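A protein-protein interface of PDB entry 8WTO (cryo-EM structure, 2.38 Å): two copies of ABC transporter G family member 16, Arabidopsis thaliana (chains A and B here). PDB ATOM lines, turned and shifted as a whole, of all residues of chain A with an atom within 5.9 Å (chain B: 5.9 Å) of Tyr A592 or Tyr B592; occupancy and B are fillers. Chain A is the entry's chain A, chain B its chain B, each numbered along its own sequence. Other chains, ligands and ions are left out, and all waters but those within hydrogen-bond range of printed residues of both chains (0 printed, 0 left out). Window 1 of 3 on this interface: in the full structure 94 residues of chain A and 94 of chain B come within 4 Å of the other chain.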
ATOM      1  N   TYR A 494     -18.160  22.999  -4.247  1.00  0.00           N
ATOM      2  CA  TYR A 494     -17.983  24.282  -4.913  1.00  0.00           C
ATOM      3  C   TYR A 494     -16.641  24.921  -4.580  1.00  0.00           C
ATOM      4  O   TYR A 494     -16.108  25.670  -5.401  1.00  0.00           O
ATOM      5  CB  TYR A 494     -19.132  25.220  -4.556  1.00  0.00           C
ATOM      6  CG  TYR A 494     -20.269  25.189  -5.543  1.00  0.00           C
ATOM      7  CD1 TYR A 494     -20.114  25.693  -6.825  1.00  0.00           C
ATOM      8  CD2 TYR A 494     -21.497  24.648  -5.195  1.00  0.00           C
ATOM      9  CE1 TYR A 494     -21.152  25.662  -7.731  1.00  0.00           C
ATOM     10  CE2 TYR A 494     -22.538  24.613  -6.091  1.00  0.00           C
ATOM     11  CZ  TYR A 494     -22.361  25.117  -7.357  1.00  0.00           C
ATOM     12  OH  TYR A 494     -23.403  25.082  -8.248  1.00  0.00           O
ATOM     13  N   ALA A 497     -13.924  23.798  -7.102  1.00  0.00           N
ATOM     14  CA  ALA A 497     -13.863  24.396  -8.425  1.00  0.00           C
ATOM     15  C   ALA A 497     -12.683  25.345  -8.586  1.00  0.00           C
ATOM     16  O   ALA A 497     -12.317  25.652  -9.720  1.00  0.00           O
ATOM     17  CB  ALA A 497     -15.168  25.124  -8.734  1.00  0.00           C
ATOM     18  N   ASP A 498     -12.044  25.778  -7.495  1.00  0.00           N
ATOM     19  CA  ASP A 498     -10.866  26.627  -7.634  1.00  0.00           C
ATOM     20  C   ASP A 498      -9.632  25.861  -8.104  1.00  0.00           C
ATOM     21  O   ASP A 498      -8.610  26.488  -8.394  1.00  0.00           O
ATOM     22  CB  ASP A 498     -10.585  27.391  -6.324  1.00  0.00           C
ATOM     23  CG  ASP A 498     -10.080  26.508  -5.168  1.00  0.00           C
ATOM     24  OD1 ASP A 498     -10.060  25.260  -5.226  1.00  0.00           O
ATOM     25  OD2 ASP A 498      -9.694  27.108  -4.148  1.00  0.00           O
ATOM     26  N   ALA A 499      -9.706  24.534  -8.180  1.00  0.00           N
ATOM     27  CA  ALA A 499      -8.650  23.707  -8.737  1.00  0.00           C
ATOM     28  C   ALA A 499      -8.650  23.684 -10.258  1.00  0.00           C
ATOM     29  O   ALA A 499      -7.725  23.117 -10.844  1.00  0.00           O
ATOM     30  CB  ALA A 499      -8.774  22.276  -8.206  1.00  0.00           C
ATOM     31  N   LEU A 500      -9.657  24.259 -10.909  1.00  0.00           N
ATOM     32  CA  LEU A 500      -9.748  24.273 -12.369  1.00  0.00           C
ATOM     33  C   LEU A 500      -8.610  25.022 -13.078  1.00  0.00           C
ATOM     34  O   LEU A 500      -8.102  24.497 -14.075  1.00  0.00           O
ATOM     35  CB  LEU A 500     -11.104  24.826 -12.824  1.00  0.00           C
ATOM     36  CG  LEU A 500     -11.362  24.584 -14.312  1.00  0.00           C
ATOM     37  CD1 LEU A 500     -12.143  23.309 -14.575  1.00  0.00           C
ATOM     38  CD2 LEU A 500     -11.991  25.774 -14.966  1.00  0.00           C
ATOM     39  N   PRO A 501      -8.145  26.202 -12.642  1.00  0.00           N
ATOM     40  CA  PRO A 501      -6.994  26.793 -13.334  1.00  0.00           C
ATOM     41  C   PRO A 501      -5.640  26.201 -12.970  1.00  0.00           C
ATOM     42  O   PRO A 501      -4.636  26.695 -13.486  1.00  0.00           O
ATOM     43  CB  PRO A 501      -7.064  28.273 -12.915  1.00  0.00           C
ATOM     44  CG  PRO A 501      -8.399  28.466 -12.378  1.00  0.00           C
ATOM     45  CD  PRO A 501      -8.696  27.202 -11.706  1.00  0.00           C
ATOM     46  N   HIS A 587     -10.256  26.160 -21.980  1.00  0.00           N
ATOM     47  CA  HIS A 587     -10.369  27.521 -21.491  1.00  0.00           C
ATOM     48  C   HIS A 587     -10.788  27.535 -20.030  1.00  0.00           C
ATOM     49  O   HIS A 587     -11.538  26.673 -19.573  1.00  0.00           O
ATOM     50  CB  HIS A 587     -11.380  28.295 -22.342  1.00  0.00           C
ATOM     51  CG  HIS A 587     -11.277  29.778 -22.210  1.00  0.00           C
ATOM     52  ND1 HIS A 587     -12.326  30.621 -22.498  1.00  0.00           N
ATOM     53  CD2 HIS A 587     -10.254  30.572 -21.813  1.00  0.00           C
ATOM     54  CE1 HIS A 587     -11.953  31.870 -22.289  1.00  0.00           C
ATOM     55  NE2 HIS A 587     -10.702  31.868 -21.869  1.00  0.00           N
ATOM     56  N   VAL A 588     -10.297  28.533 -19.298  1.00  0.00           N
ATOM     57  CA  VAL A 588     -10.670  28.655 -17.896  1.00  0.00           C
ATOM     58  C   VAL A 588     -12.105  29.168 -17.766  1.00  0.00           C
ATOM     59  O   VAL A 588     -12.802  28.831 -16.807  1.00  0.00           O
ATOM     60  CB  VAL A 588      -9.640  29.536 -17.151  1.00  0.00           C
ATOM     61  CG1 VAL A 588      -9.679  30.973 -17.617  1.00  0.00           C
ATOM     62  CG2 VAL A 588      -9.820  29.457 -15.651  1.00  0.00           C
ATOM     63  N   MET A 589     -12.593  29.934 -18.742  1.00  0.00           N
ATOM     64  CA  MET A 589     -13.955  30.445 -18.652  1.00  0.00           C
ATOM     65  C   MET A 589     -14.971  29.426 -19.144  1.00  0.00           C
ATOM     66  O   MET A 589     -16.078  29.353 -18.602  1.00  0.00           O
ATOM     67  CB  MET A 589     -14.086  31.750 -19.435  1.00  0.00           C
ATOM     68  CG  MET A 589     -13.684  32.965 -18.643  1.00  0.00           C
ATOM     69  SD  MET A 589     -14.197  34.503 -19.404  1.00  0.00           S
ATOM     70  CE  MET A 589     -12.853  34.794 -20.540  1.00  0.00           C
ATOM     71  N   LEU A 590     -14.622  28.665 -20.188  1.00  0.00           N
ATOM     72  CA  LEU A 590     -15.414  27.505 -20.584  1.00  0.00           C
ATOM     73  C   LEU A 590     -15.526  26.500 -19.451  1.00  0.00           C
ATOM     74  O   LEU A 590     -16.590  25.912 -19.236  1.00  0.00           O
ATOM     75  CB  LEU A 590     -14.796  26.814 -21.800  1.00  0.00           C
ATOM     76  CG  LEU A 590     -15.166  27.094 -23.255  1.00  0.00           C
ATOM     77  CD1 LEU A 590     -16.611  26.751 -23.502  1.00  0.00           C
ATOM     78  CD2 LEU A 590     -14.863  28.506 -23.684  1.00  0.00           C
ATOM     79  N   GLY A 591     -14.428  26.282 -18.728  1.00  0.00           N
ATOM     80  CA  GLY A 591     -14.421  25.269 -17.693  1.00  0.00           C
ATOM     81  C   GLY A 591     -15.256  25.654 -16.493  1.00  0.00           C
ATOM     82  O   GLY A 591     -15.952  24.816 -15.924  1.00  0.00           O
ATOM     83  N   TYR A 592     -15.221  26.928 -16.109  1.00  0.00           N
ATOM     84  CA  TYR A 592     -16.026  27.374 -14.981  1.00  0.00           C
ATOM     85  C   TYR A 592     -17.506  27.413 -15.319  1.00  0.00           C
ATOM     86  O   TYR A 592     -18.341  27.257 -14.428  1.00  0.00           O
ATOM     87  CB  TYR A 592     -15.544  28.735 -14.499  1.00  0.00           C
ATOM     88  CG  TYR A 592     -14.518  28.564 -13.430  1.00  0.00           C
ATOM     89  CD1 TYR A 592     -13.185  28.845 -13.671  1.00  0.00           C
ATOM     90  CD2 TYR A 592     -14.872  28.063 -12.191  1.00  0.00           C
ATOM     91  CE1 TYR A 592     -12.237  28.638 -12.708  1.00  0.00           C
ATOM     92  CE2 TYR A 592     -13.942  27.876 -11.225  1.00  0.00           C
ATOM     93  CZ  TYR A 592     -12.625  28.174 -11.482  1.00  0.00           C
ATOM     94  OH  TYR A 592     -11.682  27.989 -10.509  1.00  0.00           O
ATOM     95  N   THR A 593     -17.848  27.615 -16.588  1.00  0.00           N
ATOM     96  CA  THR A 593     -19.241  27.527 -17.000  1.00  0.00           C
ATOM     97  C   THR A 593     -19.754  26.099 -16.872  1.00  0.00           C
ATOM     98  O   THR A 593     -20.902  25.875 -16.476  1.00  0.00           O
ATOM     99  CB  THR A 593     -19.385  28.032 -18.434  1.00  0.00           C
ATOM    100  OG1 THR A 593     -18.730  29.296 -18.557  1.00  0.00           O
ATOM    101  CG2 THR A 593     -20.838  28.183 -18.817  1.00  0.00           C
ATOM    102  N   ILE A 594     -18.895  25.124 -17.150  1.00  0.00           N
ATOM    103  CA  ILE A 594     -19.309  23.729 -17.181  1.00  0.00           C
ATOM    104  C   ILE A 594     -19.269  23.109 -15.786  1.00  0.00           C
ATOM    105  O   ILE A 594     -20.183  22.371 -15.411  1.00  0.00           O
ATOM    106  CB  ILE A 594     -18.440  22.975 -18.206  1.00  0.00           C
ATOM    107  CG1 ILE A 594     -18.774  23.475 -19.608  1.00  0.00           C
ATOM    108  CG2 ILE A 594     -18.663  21.487 -18.152  1.00  0.00           C
ATOM    109  CD1 ILE A 594     -17.795  23.054 -20.665  1.00  0.00           C
ATOM    110  N   VAL A 595     -18.238  23.421 -14.988  1.00  0.00           N
ATOM    111  CA  VAL A 595     -18.114  22.882 -13.628  1.00  0.00           C
ATOM    112  C   VAL A 595     -19.265  23.346 -12.743  1.00  0.00           C
ATOM    113  O   VAL A 595     -19.866  22.549 -12.017  1.00  0.00           O
ATOM    114  CB  VAL A 595     -16.751  23.259 -13.013  1.00  0.00           C
ATOM    115  CG1 VAL A 595     -16.676  22.868 -11.557  1.00  0.00           C
ATOM    116  CG2 VAL A 595     -15.652  22.533 -13.705  1.00  0.00           C
ATOM    117  N   VAL A 596     -19.597  24.637 -12.806  1.00  0.00           N
ATOM    118  CA  VAL A 596     -20.655  25.201 -11.973  1.00  0.00           C
ATOM    119  C   VAL A 596     -22.015  24.620 -12.345  1.00  0.00           C
ATOM    120  O   VAL A 596     -22.834  24.316 -11.469  1.00  0.00           O
ATOM    121  CB  VAL A 596     -20.619  26.740 -12.075  1.00  0.00           C
ATOM    122  CG1 VAL A 596     -21.861  27.369 -11.541  1.00  0.00           C
ATOM    123  CG2 VAL A 596     -19.440  27.270 -11.300  1.00  0.00           C
ATOM    124  N   ALA A 597     -22.244  24.391 -13.639  1.00  0.00           N
ATOM    125  CA  ALA A 597     -23.496  23.799 -14.095  1.00  0.00           C
ATOM    126  C   ALA A 597     -23.633  22.347 -13.650  1.00  0.00           C
ATOM    127  O   ALA A 597     -24.706  21.936 -13.201  1.00  0.00           O
ATOM    128  CB  ALA A 597     -23.599  23.907 -15.614  1.00  0.00           C
ATOM    129  N   TYR B 494     -24.331  31.683  -9.277  1.00  0.00           N
ATOM    130  CA  TYR B 494     -23.150  30.856  -9.489  1.00  0.00           C
ATOM    131  C   TYR B 494     -22.740  30.807 -10.955  1.00  0.00           C
ATOM    132  O   TYR B 494     -21.555  30.636 -11.245  1.00  0.00           O
ATOM    133  CB  TYR B 494     -23.392  29.450  -8.947  1.00  0.00           C
ATOM    134  CG  TYR B 494     -22.920  29.257  -7.531  1.00  0.00           C
ATOM    135  CD1 TYR B 494     -21.570  29.261  -7.221  1.00  0.00           C
ATOM    136  CD2 TYR B 494     -23.829  29.079  -6.498  1.00  0.00           C
ATOM    137  CE1 TYR B 494     -21.136  29.089  -5.924  1.00  0.00           C
ATOM    138  CE2 TYR B 494     -23.407  28.906  -5.202  1.00  0.00           C
ATOM    139  CZ  TYR B 494     -22.063  28.915  -4.920  1.00  0.00           C
ATOM    140  OH  TYR B 494     -21.646  28.740  -3.625  1.00  0.00           O
ATOM    141  N   ALA B 497     -20.272  33.674 -11.784  1.00  0.00           N
ATOM    142  CA  ALA B 497     -18.874  33.567 -11.405  1.00  0.00           C
ATOM    143  C   ALA B 497     -17.959  33.323 -12.598  1.00  0.00           C
ATOM    144  O   ALA B 497     -16.754  33.545 -12.479  1.00  0.00           O
ATOM    145  CB  ALA B 497     -18.694  32.460 -10.370  1.00  0.00           C
ATOM    146  N   ASP B 498     -18.494  32.924 -13.756  1.00  0.00           N
ATOM    147  CA  ASP B 498     -17.642  32.758 -14.929  1.00  0.00           C
ATOM    148  C   ASP B 498     -17.204  34.087 -15.540  1.00  0.00           C
ATOM    149  O   ASP B 498     -16.371  34.084 -16.449  1.00  0.00           O
ATOM    150  CB  ASP B 498     -18.326  31.858 -15.977  1.00  0.00           C
ATOM    151  CG  ASP B 498     -19.537  32.504 -16.678  1.00  0.00           C
ATOM    152  OD1 ASP B 498     -20.029  33.594 -16.315  1.00  0.00           O
ATOM    153  OD2 ASP B 498     -20.016  31.872 -17.637  1.00  0.00           O
ATOM    154  N   ALA B 499     -17.745  35.206 -15.065  1.00  0.00           N
ATOM    155  CA  ALA B 499     -17.314  36.533 -15.468  1.00  0.00           C
ATOM    156  C   ALA B 499     -16.039  36.986 -14.771  1.00  0.00           C
ATOM    157  O   ALA B 499     -15.511  38.041 -15.124  1.00  0.00           O
ATOM    158  CB  ALA B 499     -18.428  37.548 -15.197  1.00  0.00           C
ATOM    159  N   LEU B 500     -15.546  36.237 -13.789  1.00  0.00           N
ATOM    160  CA  LEU B 500     -14.335  36.600 -13.053  1.00  0.00           C
ATOM    161  C   LEU B 500     -13.059  36.664 -13.905  1.00  0.00           C
ATOM    162  O   LEU B 500     -12.292  37.618 -13.730  1.00  0.00           O
ATOM    163  CB  LEU B 500     -14.124  35.661 -11.858  1.00  0.00           C
ATOM    164  CG  LEU B 500     -13.055  36.179 -10.894  1.00  0.00           C
ATOM    165  CD1 LEU B 500     -13.638  36.992  -9.751  1.00  0.00           C
ATOM    166  CD2 LEU B 500     -12.170  35.075 -10.405  1.00  0.00           C
ATOM    167  N   PRO B 501     -12.766  35.738 -14.830  1.00  0.00           N
ATOM    168  CA  PRO B 501     -11.570  35.937 -15.656  1.00  0.00           C
ATOM    169  C   PRO B 501     -11.724  36.933 -16.796  1.00  0.00           C
ATOM    170  O   PRO B 501     -10.763  37.099 -17.551  1.00  0.00           O
ATOM    171  CB  PRO B 501     -11.294  34.527 -16.206  1.00  0.00           C
ATOM    172  CG  PRO B 501     -12.071  33.623 -15.377  1.00  0.00           C
ATOM    173  CD  PRO B 501     -13.286  34.378 -15.073  1.00  0.00           C
ATOM    174  N   HIS B 587      -5.547  37.500  -8.793  1.00  0.00           N
ATOM    175  CA  HIS B 587      -5.397  36.152  -9.305  1.00  0.00           C
ATOM    176  C   HIS B 587      -6.754  35.542  -9.621  1.00  0.00           C
ATOM    177  O   HIS B 587      -7.750  35.823  -8.955  1.00  0.00           O
ATOM    178  CB  HIS B 587      -4.651  35.288  -8.284  1.00  0.00           C
ATOM    179  CG  HIS B 587      -4.078  34.033  -8.853  1.00  0.00           C
ATOM    180  ND1 HIS B 587      -3.789  32.934  -8.076  1.00  0.00           N
ATOM    181  CD2 HIS B 587      -3.747  33.695 -10.121  1.00  0.00           C
ATOM    182  CE1 HIS B 587      -3.300  31.975  -8.840  1.00  0.00           C
ATOM    183  NE2 HIS B 587      -3.268  32.408 -10.086  1.00  0.00           N
ATOM    184  N   VAL B 588      -6.783  34.697 -10.650  1.00  0.00           N
ATOM    185  CA  VAL B 588      -8.026  34.030 -11.006  1.00  0.00           C
ATOM    186  C   VAL B 588      -8.351  32.927 -10.000  1.00  0.00           C
ATOM    187  O   VAL B 588      -9.523  32.635  -9.752  1.00  0.00           O
ATOM    188  CB  VAL B 588      -7.953  33.521 -12.465  1.00  0.00           C
ATOM    189  CG1 VAL B 588      -6.939  32.412 -12.628  1.00  0.00           C
ATOM    190  CG2 VAL B 588      -9.309  33.083 -12.972  1.00  0.00           C
ATOM    191  N   MET B 589      -7.340  32.336  -9.362  1.00  0.00           N
ATOM    192  CA  MET B 589      -7.609  31.276  -8.397  1.00  0.00           C
ATOM    193  C   MET B 589      -7.954  31.838  -7.027  1.00  0.00           C
ATOM    194  O   MET B 589      -8.781  31.260  -6.317  1.00  0.00           O
ATOM    195  CB  MET B 589      -6.415  30.329  -8.301  1.00  0.00           C
ATOM    196  CG  MET B 589      -6.425  29.247  -9.348  1.00  0.00           C
ATOM    197  SD  MET B 589      -5.266  27.925  -9.005  1.00  0.00           S
ATOM    198  CE  MET B 589      -3.766  28.589  -9.703  1.00  0.00           C
ATOM    199  N   LEU B 590      -7.300  32.938  -6.632  1.00  0.00           N
ATOM    200  CA  LEU B 590      -7.719  33.690  -5.453  1.00  0.00           C
ATOM    201  C   LEU B 590      -9.152  34.174  -5.588  1.00  0.00           C
ATOM    202  O   LEU B 590      -9.918  34.145  -4.621  1.00  0.00           O
ATOM    203  CB  LEU B 590      -6.807  34.896  -5.227  1.00  0.00           C
ATOM    204  CG  LEU B 590      -5.568  34.910  -4.334  1.00  0.00           C
ATOM    205  CD1 LEU B 590      -5.953  34.639  -2.904  1.00  0.00           C
ATOM    206  CD2 LEU B 590      -4.492  33.959  -4.794  1.00  0.00           C
ATOM    207  N   GLY B 591      -9.522  34.640  -6.782  1.00  0.00           N
ATOM    208  CA  GLY B 591     -10.839  35.211  -6.970  1.00  0.00           C
ATOM    209  C   GLY B 591     -11.939  34.177  -6.924  1.00  0.00           C
ATOM    210  O   GLY B 591     -13.005  34.425  -6.367  1.00  0.00           O
ATOM    211  N   TYR B 592     -11.690  32.996  -7.486  1.00  0.00           N
ATOM    212  CA  TYR B 592     -12.693  31.941  -7.445  1.00  0.00           C
ATOM    213  C   TYR B 592     -12.845  31.355  -6.053  1.00  0.00           C
ATOM    214  O   TYR B 592     -13.922  30.866  -5.709  1.00  0.00           O
ATOM    215  CB  TYR B 592     -12.353  30.857  -8.458  1.00  0.00           C
ATOM    216  CG  TYR B 592     -13.017  31.149  -9.761  1.00  0.00           C
ATOM    217  CD1 TYR B 592     -12.282  31.566 -10.857  1.00  0.00           C
ATOM    218  CD2 TYR B 592     -14.391  31.068  -9.883  1.00  0.00           C
ATOM    219  CE1 TYR B 592     -12.895  31.884 -12.037  1.00  0.00           C
ATOM    220  CE2 TYR B 592     -15.005  31.363 -11.055  1.00  0.00           C
ATOM    221  CZ  TYR B 592     -14.253  31.760 -12.134  1.00  0.00           C
ATOM    222  OH  TYR B 592     -14.867  32.055 -13.320  1.00  0.00           O
ATOM    223  N   THR B 593     -11.789  31.393  -5.245  1.00  0.00           N
ATOM    224  CA  THR B 593     -11.907  30.972  -3.857  1.00  0.00           C
ATOM    225  C   THR B 593     -12.799  31.926  -3.076  1.00  0.00           C
ATOM    226  O   THR B 593     -13.582  31.499  -2.222  1.00  0.00           O
ATOM    227  CB  THR B 593     -10.517  30.886  -3.229  1.00  0.00           C
ATOM    228  OG1 THR B 593      -9.658  30.131  -4.085  1.00  0.00           O
ATOM    229  CG2 THR B 593     -10.571  30.227  -1.870  1.00  0.00           C
ATOM    230  N   ILE B 594     -12.729  33.214  -3.396  1.00  0.00           N
ATOM    231  CA  ILE B 594     -13.444  34.228  -2.637  1.00  0.00           C
ATOM    232  C   ILE B 594     -14.883  34.378  -3.129  1.00  0.00           C
ATOM    233  O   ILE B 594     -15.802  34.496  -2.317  1.00  0.00           O
ATOM    234  CB  ILE B 594     -12.642  35.544  -2.689  1.00  0.00           C
ATOM    235  CG1 ILE B 594     -11.342  35.368  -1.913  1.00  0.00           C
ATOM    236  CG2 ILE B 594     -13.410  36.698  -2.104  1.00  0.00           C
ATOM    237  CD1 ILE B 594     -10.334  36.456  -2.140  1.00  0.00           C
ATOM    238  N   VAL B 595     -15.101  34.339  -4.450  1.00  0.00           N
ATOM    239  CA  VAL B 595     -16.448  34.469  -5.020  1.00  0.00           C
ATOM    240  C   VAL B 595     -17.344  33.314  -4.587  1.00  0.00           C
ATOM    241  O   VAL B 595     -18.492  33.521  -4.185  1.00  0.00           O
ATOM    242  CB  VAL B 595     -16.382  34.581  -6.557  1.00  0.00           C
ATOM    243  CG1 VAL B 595     -17.759  34.526  -7.173  1.00  0.00           C
ATOM    244  CG2 VAL B 595     -15.792  35.891  -6.952  1.00  0.00           C
ATOM    245  N   VAL B 596     -16.824  32.088  -4.646  1.00  0.00           N
ATOM    246  CA  VAL B 596     -17.603  30.903  -4.291  1.00  0.00           C
ATOM    247  C   VAL B 596     -17.962  30.910  -2.809  1.00  0.00           C
ATOM    248  O   VAL B 596     -19.088  30.561  -2.429  1.00  0.00           O
ATOM    249  CB  VAL B 596     -16.828  29.636  -4.709  1.00  0.00           C
ATOM    250  CG1 VAL B 596     -17.384  28.406  -4.081  1.00  0.00           C
ATOM    251  CG2 VAL B 596     -16.890  29.477  -6.207  1.00  0.00           C
ATOM    252  N   ALA B 597     -17.041  31.372  -1.962  1.00  0.00           N
ATOM    253  CA  ALA B 597     -17.302  31.454  -0.529  1.00  0.00           C
ATOM    254  C   ALA B 597     -18.357  32.504  -0.203  1.00  0.00           C
ATOM    255  O   ALA B 597     -19.248  32.253   0.612  1.00  0.00           O
ATOM    256  CB  ALA B 597     -16.003  31.748   0.219  1.00  0.00           C
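The backbone carbonyl oxygen of Val A596 is in hydrogen-bond range of the side-chain hydroxyl of Tyr A494, 3.4 Å away.
O of Ala A497 lies within hydrogen-bond range of OH of Tyr A592 (2.5 Å).
O of Met A589 is in hydrogen-bond range of OG1 of Thr A593.
OH of Tyr B494 is in hydrogen-bond range of O of Val B596, at 3.4 Å.
The backbone carbonyl oxygen (O) of Ala B497 sits at hydrogen-bond distance from the side-chain hydroxyl (OH) of Tyr B592, 2.5 Å away.
O of Met B589 sits at hydrogen-bond distance from OG1 of Thr B593 (2.7 Å).
Among the printed residues, merely in contact across the chains: Val A596 with Tyr B494 (3.3 Å), Tyr A494 with Val B596 (3.3 Å), Tyr A592 with Tyr B592 (3.4 Å), Tyr A494 with Tyr B494 (3.7 Å), Pro A501 with Met B589 (3.7 Å) and Met A589 with Pro B501 (3.7 Å).
Tyr A494 touches its own counterpart, Tyr B494.
Tyr A494 touches Val B596, and with the chains exchanged Val A596 touches Tyr B494.
Asp A498 touches Thr B593, and with the chains exchanged Thr A593 touches Asp B498.
Pro A501 touches Met B589, and with the chains exchanged Met A589 touches Pro B501.
Of the 10 pairs that touch across the chains among the printed residues, 10 have their exchanged pair printed and touching as well.
The side-chain hydroxyl of Thr B593 is in hydrogen-bond range of the side-chain carboxylate of Asp A498 (3.0 Å).
OG1 of Thr A593 sits at hydrogen-bond distance from OD2 of Asp B498.
The side-chain sulfur of Met B589 lies close to the backbone carbonyl oxygen of Asp A498 (3.7 Å).
The backbone carbonyl oxygen of Asp B498 sits close to the side-chain sulfur of Met A589.
Hydrophobic or aromatic side chains of chain A that line the printed part of chain B: Tyr A494, Pro A501, Met A589, Tyr A592 and Val A596.
Along chain A the printed residues that touch a printed residue of chain B span positions 494 to 596.
Of the 17 printed residues of chain B, 7 touch a printed residue of chain A.
Among the printed residues, no Asp or Glu carboxylate lies within 4 Å of a Lys or Arg side-chain nitrogen of the other chain.
Of the printed residues of chain B, Pro A501 touches Met B589.
Tyr A592 touches just one residue of chain B: Tyr B592.
Val A595 touches none of the printed residues of chain B.
Of the printed residues of chain B, Val A596 touches Tyr B494.
Of the printed residues of chain A, Tyr B494 touches Tyr A494 (3.7 Å) and Val A596 (3.3 Å).
Gly B591 touches none of the printed residues of chain A.
Of chain A, only Tyr A592 (3.4 Å) comes within 4 Å of Tyr B592.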
